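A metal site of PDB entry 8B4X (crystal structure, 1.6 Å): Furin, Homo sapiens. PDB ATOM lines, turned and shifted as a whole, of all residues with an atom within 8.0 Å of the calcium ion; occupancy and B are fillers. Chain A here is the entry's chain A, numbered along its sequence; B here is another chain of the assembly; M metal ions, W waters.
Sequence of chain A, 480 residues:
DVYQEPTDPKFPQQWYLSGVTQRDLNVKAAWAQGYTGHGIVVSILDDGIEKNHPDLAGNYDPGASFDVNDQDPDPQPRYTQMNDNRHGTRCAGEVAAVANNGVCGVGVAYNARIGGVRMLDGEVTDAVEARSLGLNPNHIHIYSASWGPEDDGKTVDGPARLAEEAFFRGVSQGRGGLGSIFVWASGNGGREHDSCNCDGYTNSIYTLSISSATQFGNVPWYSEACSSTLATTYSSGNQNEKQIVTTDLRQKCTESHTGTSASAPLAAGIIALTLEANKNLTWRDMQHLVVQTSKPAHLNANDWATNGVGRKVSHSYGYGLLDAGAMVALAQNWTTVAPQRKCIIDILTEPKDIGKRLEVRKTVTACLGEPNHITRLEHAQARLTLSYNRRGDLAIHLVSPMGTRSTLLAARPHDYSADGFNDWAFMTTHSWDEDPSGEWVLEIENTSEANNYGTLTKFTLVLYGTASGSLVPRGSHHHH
The backbone carbonyl oxygen of Gly 189 lies within hydrogen-bond range of the backbone NH of Asp 194 (3.0 Å).
OD1 of Asp 194 is in salt-bridge range of NH1 of Arg 412, 2.9 Å away.
The side-chain carboxylate (OD1) of Asp 151 lies close to NBU of OZ3 5 of chain B, at 3.8 Å.
The side-chain carboxylate (OD2) of Asp 151 is in hydrogen-bond range of the backbone NH (N) of Asn 188, 2.9 Å away.
N of Gly 189 sits close to OE2 of Glu 224, at 2.8 Å.
The side-chain carboxylate of Glu 224 sits close to the backbone NH of Cys 196, at 3.3 Å.
The side-chain carboxylate (OE2) of Glu 224 sits close to the backbone NH (N) of Asn 188 (3.3 Å).
Of the 27 residues printed, 3 come within 4 Å of the calcium ion.
The calcium ion is bound by the side-chain carboxylate (OD2) of Asp 194, the side-chain carboxylate (OD1) of Asp 151, water W2, the side-chain carboxylate (OE2) of Glu 224, water W1, water W3 and the side-chain carboxylate (OE1) of Glu 224.
The calcium ion has seven donor atoms within binding distance.
Water W2 lies within hydrogen-bond range of the backbone carbonyl oxygen of Ser 186 (2.7 Å), the side-chain carboxylate of Asp 199 (2.7 Å) and NBU of OZ3 5 of chain B (3.4 Å).
Water W3 lies within hydrogen-bond range of the backbone carbonyl oxygen (O) of Ser 195 (2.7 Å) and the side-chain carboxylate (OD1) of Asp 194 (3.4 Å).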
ATOM      1  N   GLY A 148     -29.901  30.147  13.260  1.00  0.00           N
ATOM      2  CA  GLY A 148     -29.398  28.813  13.143  1.00  0.00           C
ATOM      3  C   GLY A 148     -27.909  28.746  13.389  1.00  0.00           C
ATOM      4  O   GLY A 148     -27.297  29.659  13.942  1.00  0.00           O
ATOM      5  N   PRO A 149     -27.302  27.635  12.965  1.00  0.00           N
ATOM      6  CA  PRO A 149     -25.859  27.475  13.157  1.00  0.00           C
ATOM      7  C   PRO A 149     -25.086  28.535  12.374  1.00  0.00           C
ATOM      8  O   PRO A 149     -25.599  29.116  11.413  1.00  0.00           O
ATOM      9  CB  PRO A 149     -25.567  26.077  12.622  1.00  0.00           C
ATOM     10  CG  PRO A 149     -26.880  25.399  12.549  1.00  0.00           C
ATOM     11  CD  PRO A 149     -27.932  26.442  12.382  1.00  0.00           C
ATOM     12  N   GLU A 150     -23.829  28.742  12.775  1.00  0.00           N
ATOM     13  CA  GLU A 150     -23.019  29.803  12.190  1.00  0.00           C
ATOM     14  C   GLU A 150     -22.925  29.668  10.679  1.00  0.00           C
ATOM     15  O   GLU A 150     -22.746  28.572  10.140  1.00  0.00           O
ATOM     16  CB  GLU A 150     -21.621  29.793  12.820  1.00  0.00           C
ATOM     17  CG  GLU A 150     -20.792  31.036  12.489  1.00  0.00           C
ATOM     18  CD  GLU A 150     -19.554  31.216  13.353  1.00  0.00           C
ATOM     19  OE1 GLU A 150     -19.404  30.489  14.352  1.00  0.00           O
ATOM     20  OE2 GLU A 150     -18.724  32.101  13.022  1.00  0.00           O
ATOM     21  N   ASP A 151     -23.085  30.799   9.992  1.00  0.00           N
ATOM     22  CA  ASP A 151     -22.958  30.918   8.540  1.00  0.00           C
ATOM     23  C   ASP A 151     -21.525  31.215   8.120  1.00  0.00           C
ATOM     24  O   ASP A 151     -21.284  32.064   7.256  1.00  0.00           O
ATOM     25  CB  ASP A 151     -23.883  32.026   8.043  1.00  0.00           C
ATOM     26  CG  ASP A 151     -25.349  31.632   8.096  1.00  0.00           C
ATOM     27  OD1 ASP A 151     -25.626  30.423   7.996  1.00  0.00           O
ATOM     28  OD2 ASP A 151     -26.227  32.540   8.211  1.00  0.00           O
ATOM     29  N   ASP A 152     -20.529  30.565   8.740  1.00  0.00           N
ATOM     30  CA  ASP A 152     -19.150  30.820   8.360  1.00  0.00           C
ATOM     31  C   ASP A 152     -18.722  29.990   7.154  1.00  0.00           C
ATOM     32  O   ASP A 152     -17.587  30.139   6.692  1.00  0.00           O
ATOM     33  CB  ASP A 152     -18.198  30.581   9.543  1.00  0.00           C
ATOM     34  CG  ASP A 152     -18.389  29.241  10.223  1.00  0.00           C
ATOM     35  OD1 ASP A 152     -19.136  28.377   9.701  1.00  0.00           O
ATOM     36  OD2 ASP A 152     -17.760  29.035  11.281  1.00  0.00           O
ATOM     37  N   GLY A 153     -19.595  29.142   6.624  1.00  0.00           N
ATOM     38  CA  GLY A 153     -19.239  28.277   5.521  1.00  0.00           C
ATOM     39  C   GLY A 153     -18.320  27.134   5.895  1.00  0.00           C
ATOM     40  O   GLY A 153     -17.729  26.512   4.999  1.00  0.00           O
ATOM     41  N   LYS A 154     -18.162  26.858   7.182  1.00  0.00           N
ATOM     42  CA  LYS A 154     -17.377  25.717   7.613  1.00  0.00           C
ATOM     43  C   LYS A 154     -18.085  24.854   8.637  1.00  0.00           C
ATOM     44  O   LYS A 154     -17.564  23.796   9.007  1.00  0.00           O
ATOM     45  CB  LYS A 154     -16.026  26.155   8.197  1.00  0.00           C
ATOM     46  CG  LYS A 154     -16.114  27.124   9.347  1.00  0.00           C
ATOM     47  N   THR A 155     -19.266  25.255   9.102  1.00  0.00           N
ATOM     48  CA  THR A 155     -19.951  24.557  10.169  1.00  0.00           C
ATOM     49  C   THR A 155     -20.886  23.492   9.593  1.00  0.00           C
ATOM     50  O   THR A 155     -21.524  23.701   8.568  1.00  0.00           O
ATOM     51  CB  THR A 155     -20.729  25.587  10.987  1.00  0.00           C
ATOM     52  OG1 THR A 155     -19.797  26.478  11.616  1.00  0.00           O
ATOM     53  CG2 THR A 155     -21.566  24.938  12.037  1.00  0.00           C
ATOM     54  N   ALA A 185     -35.846  30.114   8.112  1.00  0.00           N
ATOM     55  CA  ALA A 185     -35.054  30.876   7.147  1.00  0.00           C
ATOM     56  C   ALA A 185     -33.825  30.064   6.750  1.00  0.00           C
ATOM     57  O   ALA A 185     -33.133  29.524   7.609  1.00  0.00           O
ATOM     58  CB  ALA A 185     -34.636  32.211   7.744  1.00  0.00           C
ATOM     59  N   SER A 186     -33.533  30.016   5.444  1.00  0.00           N
ATOM     60  CA  SER A 186     -32.512  29.072   4.997  1.00  0.00           C
ATOM     61  C   SER A 186     -31.075  29.502   5.303  1.00  0.00           C
ATOM     62  O   SER A 186     -30.183  28.645   5.284  1.00  0.00           O
ATOM     63  CB  SER A 186     -32.651  28.802   3.492  1.00  0.00           C
ATOM     64  OG  SER A 186     -32.427  29.960   2.716  1.00  0.00           O
ATOM     65  N   GLY A 187     -30.828  30.783   5.586  1.00  0.00           N
ATOM     66  CA  GLY A 187     -29.488  31.191   6.018  1.00  0.00           C
ATOM     67  C   GLY A 187     -28.922  32.409   5.317  1.00  0.00           C
ATOM     68  O   GLY A 187     -29.383  32.764   4.225  1.00  0.00           O
ATOM     69  N   ASN A 188     -27.916  33.052   5.925  1.00  0.00           N
ATOM     70  CA  ASN A 188     -27.310  34.263   5.361  1.00  0.00           C
ATOM     71  C   ASN A 188     -25.840  34.052   4.978  1.00  0.00           C
ATOM     72  O   ASN A 188     -25.074  35.019   4.921  1.00  0.00           O
ATOM     73  CB  ASN A 188     -27.425  35.421   6.341  1.00  0.00           C
ATOM     74  CG  ASN A 188     -28.799  36.054   6.348  1.00  0.00           C
ATOM     75  OD1 ASN A 188     -29.582  35.889   5.416  1.00  0.00           O
ATOM     76  ND2 ASN A 188     -29.104  36.763   7.424  1.00  0.00           N
ATOM     77  N   GLY A 189     -25.438  32.823   4.682  1.00  0.00           N
ATOM     78  CA  GLY A 189     -24.030  32.531   4.473  1.00  0.00           C
ATOM     79  C   GLY A 189     -23.543  32.593   3.030  1.00  0.00           C
ATOM     80  O   GLY A 189     -22.494  32.024   2.706  1.00  0.00           O
ATOM     81  N   GLY A 190     -24.278  33.296   2.169  1.00  0.00           N
ATOM     82  CA  GLY A 190     -23.926  33.334   0.764  1.00  0.00           C
ATOM     83  C   GLY A 190     -22.524  33.842   0.497  1.00  0.00           C
ATOM     84  O   GLY A 190     -21.816  33.333  -0.378  1.00  0.00           O
ATOM     85  N   HIS A 193     -20.026  31.251   0.744  1.00  0.00           N
ATOM     86  CA  HIS A 193     -20.330  30.068  -0.059  1.00  0.00           C
ATOM     87  C   HIS A 193     -20.839  28.917   0.821  1.00  0.00           C
ATOM     88  O   HIS A 193     -20.545  27.741   0.588  1.00  0.00           O
ATOM     89  CB  HIS A 193     -19.104  29.650  -0.868  1.00  0.00           C
ATOM     90  CG  HIS A 193     -18.653  30.711  -1.820  1.00  0.00           C
ATOM     91  ND1 HIS A 193     -19.227  30.896  -3.055  1.00  0.00           N
ATOM     92  CD2 HIS A 193     -17.721  31.687  -1.689  1.00  0.00           C
ATOM     93  CE1 HIS A 193     -18.657  31.931  -3.662  1.00  0.00           C
ATOM     94  NE2 HIS A 193     -17.742  32.423  -2.846  1.00  0.00           N
ATOM     95  N   ASP A 194     -21.657  29.255   1.802  1.00  0.00           N
ATOM     96  CA  ASP A 194     -22.242  28.262   2.692  1.00  0.00           C
ATOM     97  C   ASP A 194     -23.307  27.447   1.966  1.00  0.00           C
ATOM     98  O   ASP A 194     -23.868  27.874   0.947  1.00  0.00           O
ATOM     99  CB  ASP A 194     -22.831  28.980   3.909  1.00  0.00           C
ATOM    100  CG  ASP A 194     -22.978  28.070   5.131  1.00  0.00           C
ATOM    101  OD1 ASP A 194     -22.465  26.929   5.118  1.00  0.00           O
ATOM    102  OD2 ASP A 194     -23.605  28.539   6.114  1.00  0.00           O
ATOM    103  N   SER A 195     -23.581  26.257   2.503  1.00  0.00           N
ATOM    104  CA  SER A 195     -24.619  25.366   1.999  1.00  0.00           C
ATOM    105  C   SER A 195     -25.669  25.153   3.070  1.00  0.00           C
ATOM    106  O   SER A 195     -25.342  24.745   4.193  1.00  0.00           O
ATOM    107  CB  SER A 195     -24.051  23.993   1.595  1.00  0.00           C
ATOM    108  OG  SER A 195     -25.083  23.024   1.508  1.00  0.00           O
ATOM    109  N   CYS A 196     -26.929  25.392   2.738  1.00  0.00           N
ATOM    110  CA  CYS A 196     -27.974  25.206   3.733  1.00  0.00           C
ATOM    111  C   CYS A 196     -28.301  23.727   3.978  1.00  0.00           C
ATOM    112  O   CYS A 196     -29.107  23.424   4.849  1.00  0.00           O
ATOM    113  CB  CYS A 196     -29.231  26.014   3.369  1.00  0.00           C
ATOM    114  SG  CYS A 196     -29.669  26.153   1.610  1.00  0.00           S
ATOM    115  N   ASN A 197     -27.647  22.791   3.271  1.00  0.00           N
ATOM    116  CA  ASN A 197     -27.762  21.399   3.682  1.00  0.00           C
ATOM    117  C   ASN A 197     -26.827  21.052   4.839  1.00  0.00           C
ATOM    118  O   ASN A 197     -26.950  19.952   5.414  1.00  0.00           O
ATOM    119  CB  ASN A 197     -27.477  20.463   2.513  1.00  0.00           C
ATOM    120  CG  ASN A 197     -28.646  20.358   1.555  1.00  0.00           C
ATOM    121  OD1 ASN A 197     -29.716  20.940   1.769  1.00  0.00           O
ATOM    122  ND2 ASN A 197     -28.433  19.649   0.454  1.00  0.00           N
ATOM    123  N   CYS A 198     -25.897  21.939   5.196  1.00  0.00           N
ATOM    124  CA  CYS A 198     -25.007  21.737   6.333  1.00  0.00           C
ATOM    125  C   CYS A 198     -25.577  22.307   7.626  1.00  0.00           C
ATOM    126  O   CYS A 198     -24.864  22.415   8.620  1.00  0.00           O
ATOM    127  CB  CYS A 198     -23.650  22.362   6.040  1.00  0.00           C
ATOM    128  SG  CYS A 198     -22.744  21.444   4.769  1.00  0.00           S
ATOM    129  N   ASP A 199     -26.851  22.687   7.591  1.00  0.00           N
ATOM    130  CA  ASP A 199     -27.621  23.237   8.693  1.00  0.00           C
ATOM    131  C   ASP A 199     -28.776  22.261   8.902  1.00  0.00           C
ATOM    132  O   ASP A 199     -29.630  22.112   8.025  1.00  0.00           O
ATOM    133  CB  ASP A 199     -28.062  24.654   8.291  1.00  0.00           C
ATOM    134  CG  ASP A 199     -29.022  25.310   9.241  1.00  0.00           C
ATOM    135  OD1 ASP A 199     -29.722  24.625  10.004  1.00  0.00           O
ATOM    136  OD2 ASP A 199     -29.109  26.563   9.152  1.00  0.00           O
ATOM    137  N   THR A 202     -32.601  23.675   8.712  1.00  0.00           N
ATOM    138  CA  THR A 202     -33.164  23.879   7.390  1.00  0.00           C
ATOM    139  C   THR A 202     -33.268  22.563   6.629  1.00  0.00           C
ATOM    140  O   THR A 202     -34.257  22.296   5.940  1.00  0.00           O
ATOM    141  CB  THR A 202     -32.310  24.905   6.642  1.00  0.00           C
ATOM    142  OG1 THR A 202     -30.927  24.513   6.711  1.00  0.00           O
ATOM    143  CG2 THR A 202     -32.422  26.298   7.286  1.00  0.00           C
ATOM    144  N   TYR A 222     -26.567  37.257   0.089  1.00  0.00           N
ATOM    145  CA  TYR A 222     -26.522  36.468   1.310  1.00  0.00           C
ATOM    146  C   TYR A 222     -27.084  35.056   1.140  1.00  0.00           C
ATOM    147  O   TYR A 222     -26.992  34.249   2.068  1.00  0.00           O
ATOM    148  CB  TYR A 222     -27.288  37.180   2.467  1.00  0.00           C
ATOM    149  CG  TYR A 222     -28.668  37.636   2.056  1.00  0.00           C
ATOM    150  CD1 TYR A 222     -29.741  36.757   2.062  1.00  0.00           C
ATOM    151  CD2 TYR A 222     -28.894  38.942   1.639  1.00  0.00           C
ATOM    152  CE1 TYR A 222     -30.994  37.157   1.651  1.00  0.00           C
ATOM    153  CE2 TYR A 222     -30.142  39.343   1.220  1.00  0.00           C
ATOM    154  CZ  TYR A 222     -31.196  38.444   1.233  1.00  0.00           C
ATOM    155  OH  TYR A 222     -32.459  38.810   0.831  1.00  0.00           O
ATOM    156  N   GLU A 224     -27.944  31.225   0.451  1.00  0.00           N
ATOM    157  CA  GLU A 224     -27.293  29.923   0.406  1.00  0.00           C
ATOM    158  C   GLU A 224     -28.099  29.003  -0.491  1.00  0.00           C
ATOM    159  O   GLU A 224     -29.320  28.907  -0.347  1.00  0.00           O
ATOM    160  CB  GLU A 224     -27.186  29.295   1.795  1.00  0.00           C
ATOM    161  CG  GLU A 224     -26.455  30.139   2.794  1.00  0.00           C
ATOM    162  CD  GLU A 224     -26.379  29.502   4.173  1.00  0.00           C
ATOM    163  OE1 GLU A 224     -26.259  28.263   4.250  1.00  0.00           O
ATOM    164  OE2 GLU A 224     -26.412  30.241   5.169  1.00  0.00           O
ATOM    165  N   ARG A 412     -17.266  24.113  -0.428  1.00  0.00           N
ATOM    166  CA  ARG A 412     -17.263  25.165   0.595  1.00  0.00           C
ATOM    167  C   ARG A 412     -15.819  25.564   0.849  1.00  0.00           C
ATOM    168  O   ARG A 412     -15.086  24.868   1.587  1.00  0.00           O
ATOM    169  CB  ARG A 412     -17.931  24.687   1.887  1.00  0.00           C
ATOM    170  CG  ARG A 412     -19.444  24.515   1.752  1.00  0.00           C
ATOM    171  CD  ARG A 412     -20.175  24.699   3.089  1.00  0.00           C
ATOM    172  NE  ARG A 412     -19.731  23.711   4.077  1.00  0.00           N
ATOM    173  CZ  ARG A 412     -20.038  23.751   5.371  1.00  0.00           C
ATOM    174  NH1 ARG A 412     -20.818  24.684   5.868  1.00  0.00           N
ATOM    175  NH2 ARG A 412     -19.518  22.834   6.182  1.00  0.00           N
ATOM    176  N   TBG B   3     -26.845  31.901  15.621  1.00  0.00           N
ATOM    177  CA  TBG B   3     -26.783  33.301  15.164  1.00  0.00           C
ATOM    178  CB  TBG B   3     -25.587  33.412  14.167  1.00  0.00           C
ATOM    179  CG1 TBG B   3     -24.319  32.879  14.828  1.00  0.00           C
ATOM    180  CG2 TBG B   3     -25.836  32.630  12.882  1.00  0.00           C
ATOM    181  CG3 TBG B   3     -25.382  34.876  13.774  1.00  0.00           C
ATOM    182  C   TBG B   3     -28.080  33.742  14.498  1.00  0.00           C
ATOM    183  O   TBG B   3     -28.742  32.966  13.821  1.00  0.00           O
ATOM    184  CA  OZ3 B   5     -30.185  35.307  10.295  1.00  0.00           C
ATOM    185  CBO OZ3 B   5     -30.164  33.779  10.025  1.00  0.00           C
ATOM    186  CBP OZ3 B   5     -31.293  33.138   9.532  1.00  0.00           C
ATOM    187  CBQ OZ3 B   5     -31.265  31.750   9.325  1.00  0.00           C
ATOM    188  CBR OZ3 B   5     -30.156  31.046   9.601  1.00  0.00           C
ATOM    189  CBS OZ3 B   5     -29.912  29.718   9.495  1.00  0.00           C
ATOM    190  CBV OZ3 B   5     -28.013  30.604  10.350  1.00  0.00           C
ATOM    191  CBW OZ3 B   5     -29.081  31.663  10.101  1.00  0.00           C
ATOM    192  CBX OZ3 B   5     -29.046  32.991  10.312  1.00  0.00           C
ATOM    193  N   OZ3 B   5     -30.349  35.408  11.763  1.00  0.00           N
ATOM    194  NBT OZ3 B   5     -30.722  28.760   9.018  1.00  0.00           N
ATOM    195  NBU OZ3 B   5     -28.695  29.383   9.934  1.00  0.00           N
HETATM  196 CA    CA M   1     -25.842  28.449   6.690  1.00  0.00          CA
HETATM  197  O   HOH W   1     -25.620  27.697   8.980  1.00  0.00           O
HETATM  198  O   HOH W   2     -28.174  27.883   6.938  1.00  0.00           O
HETATM  199  O   HOH W   3     -25.396  26.042   6.558  1.00  0.00           O
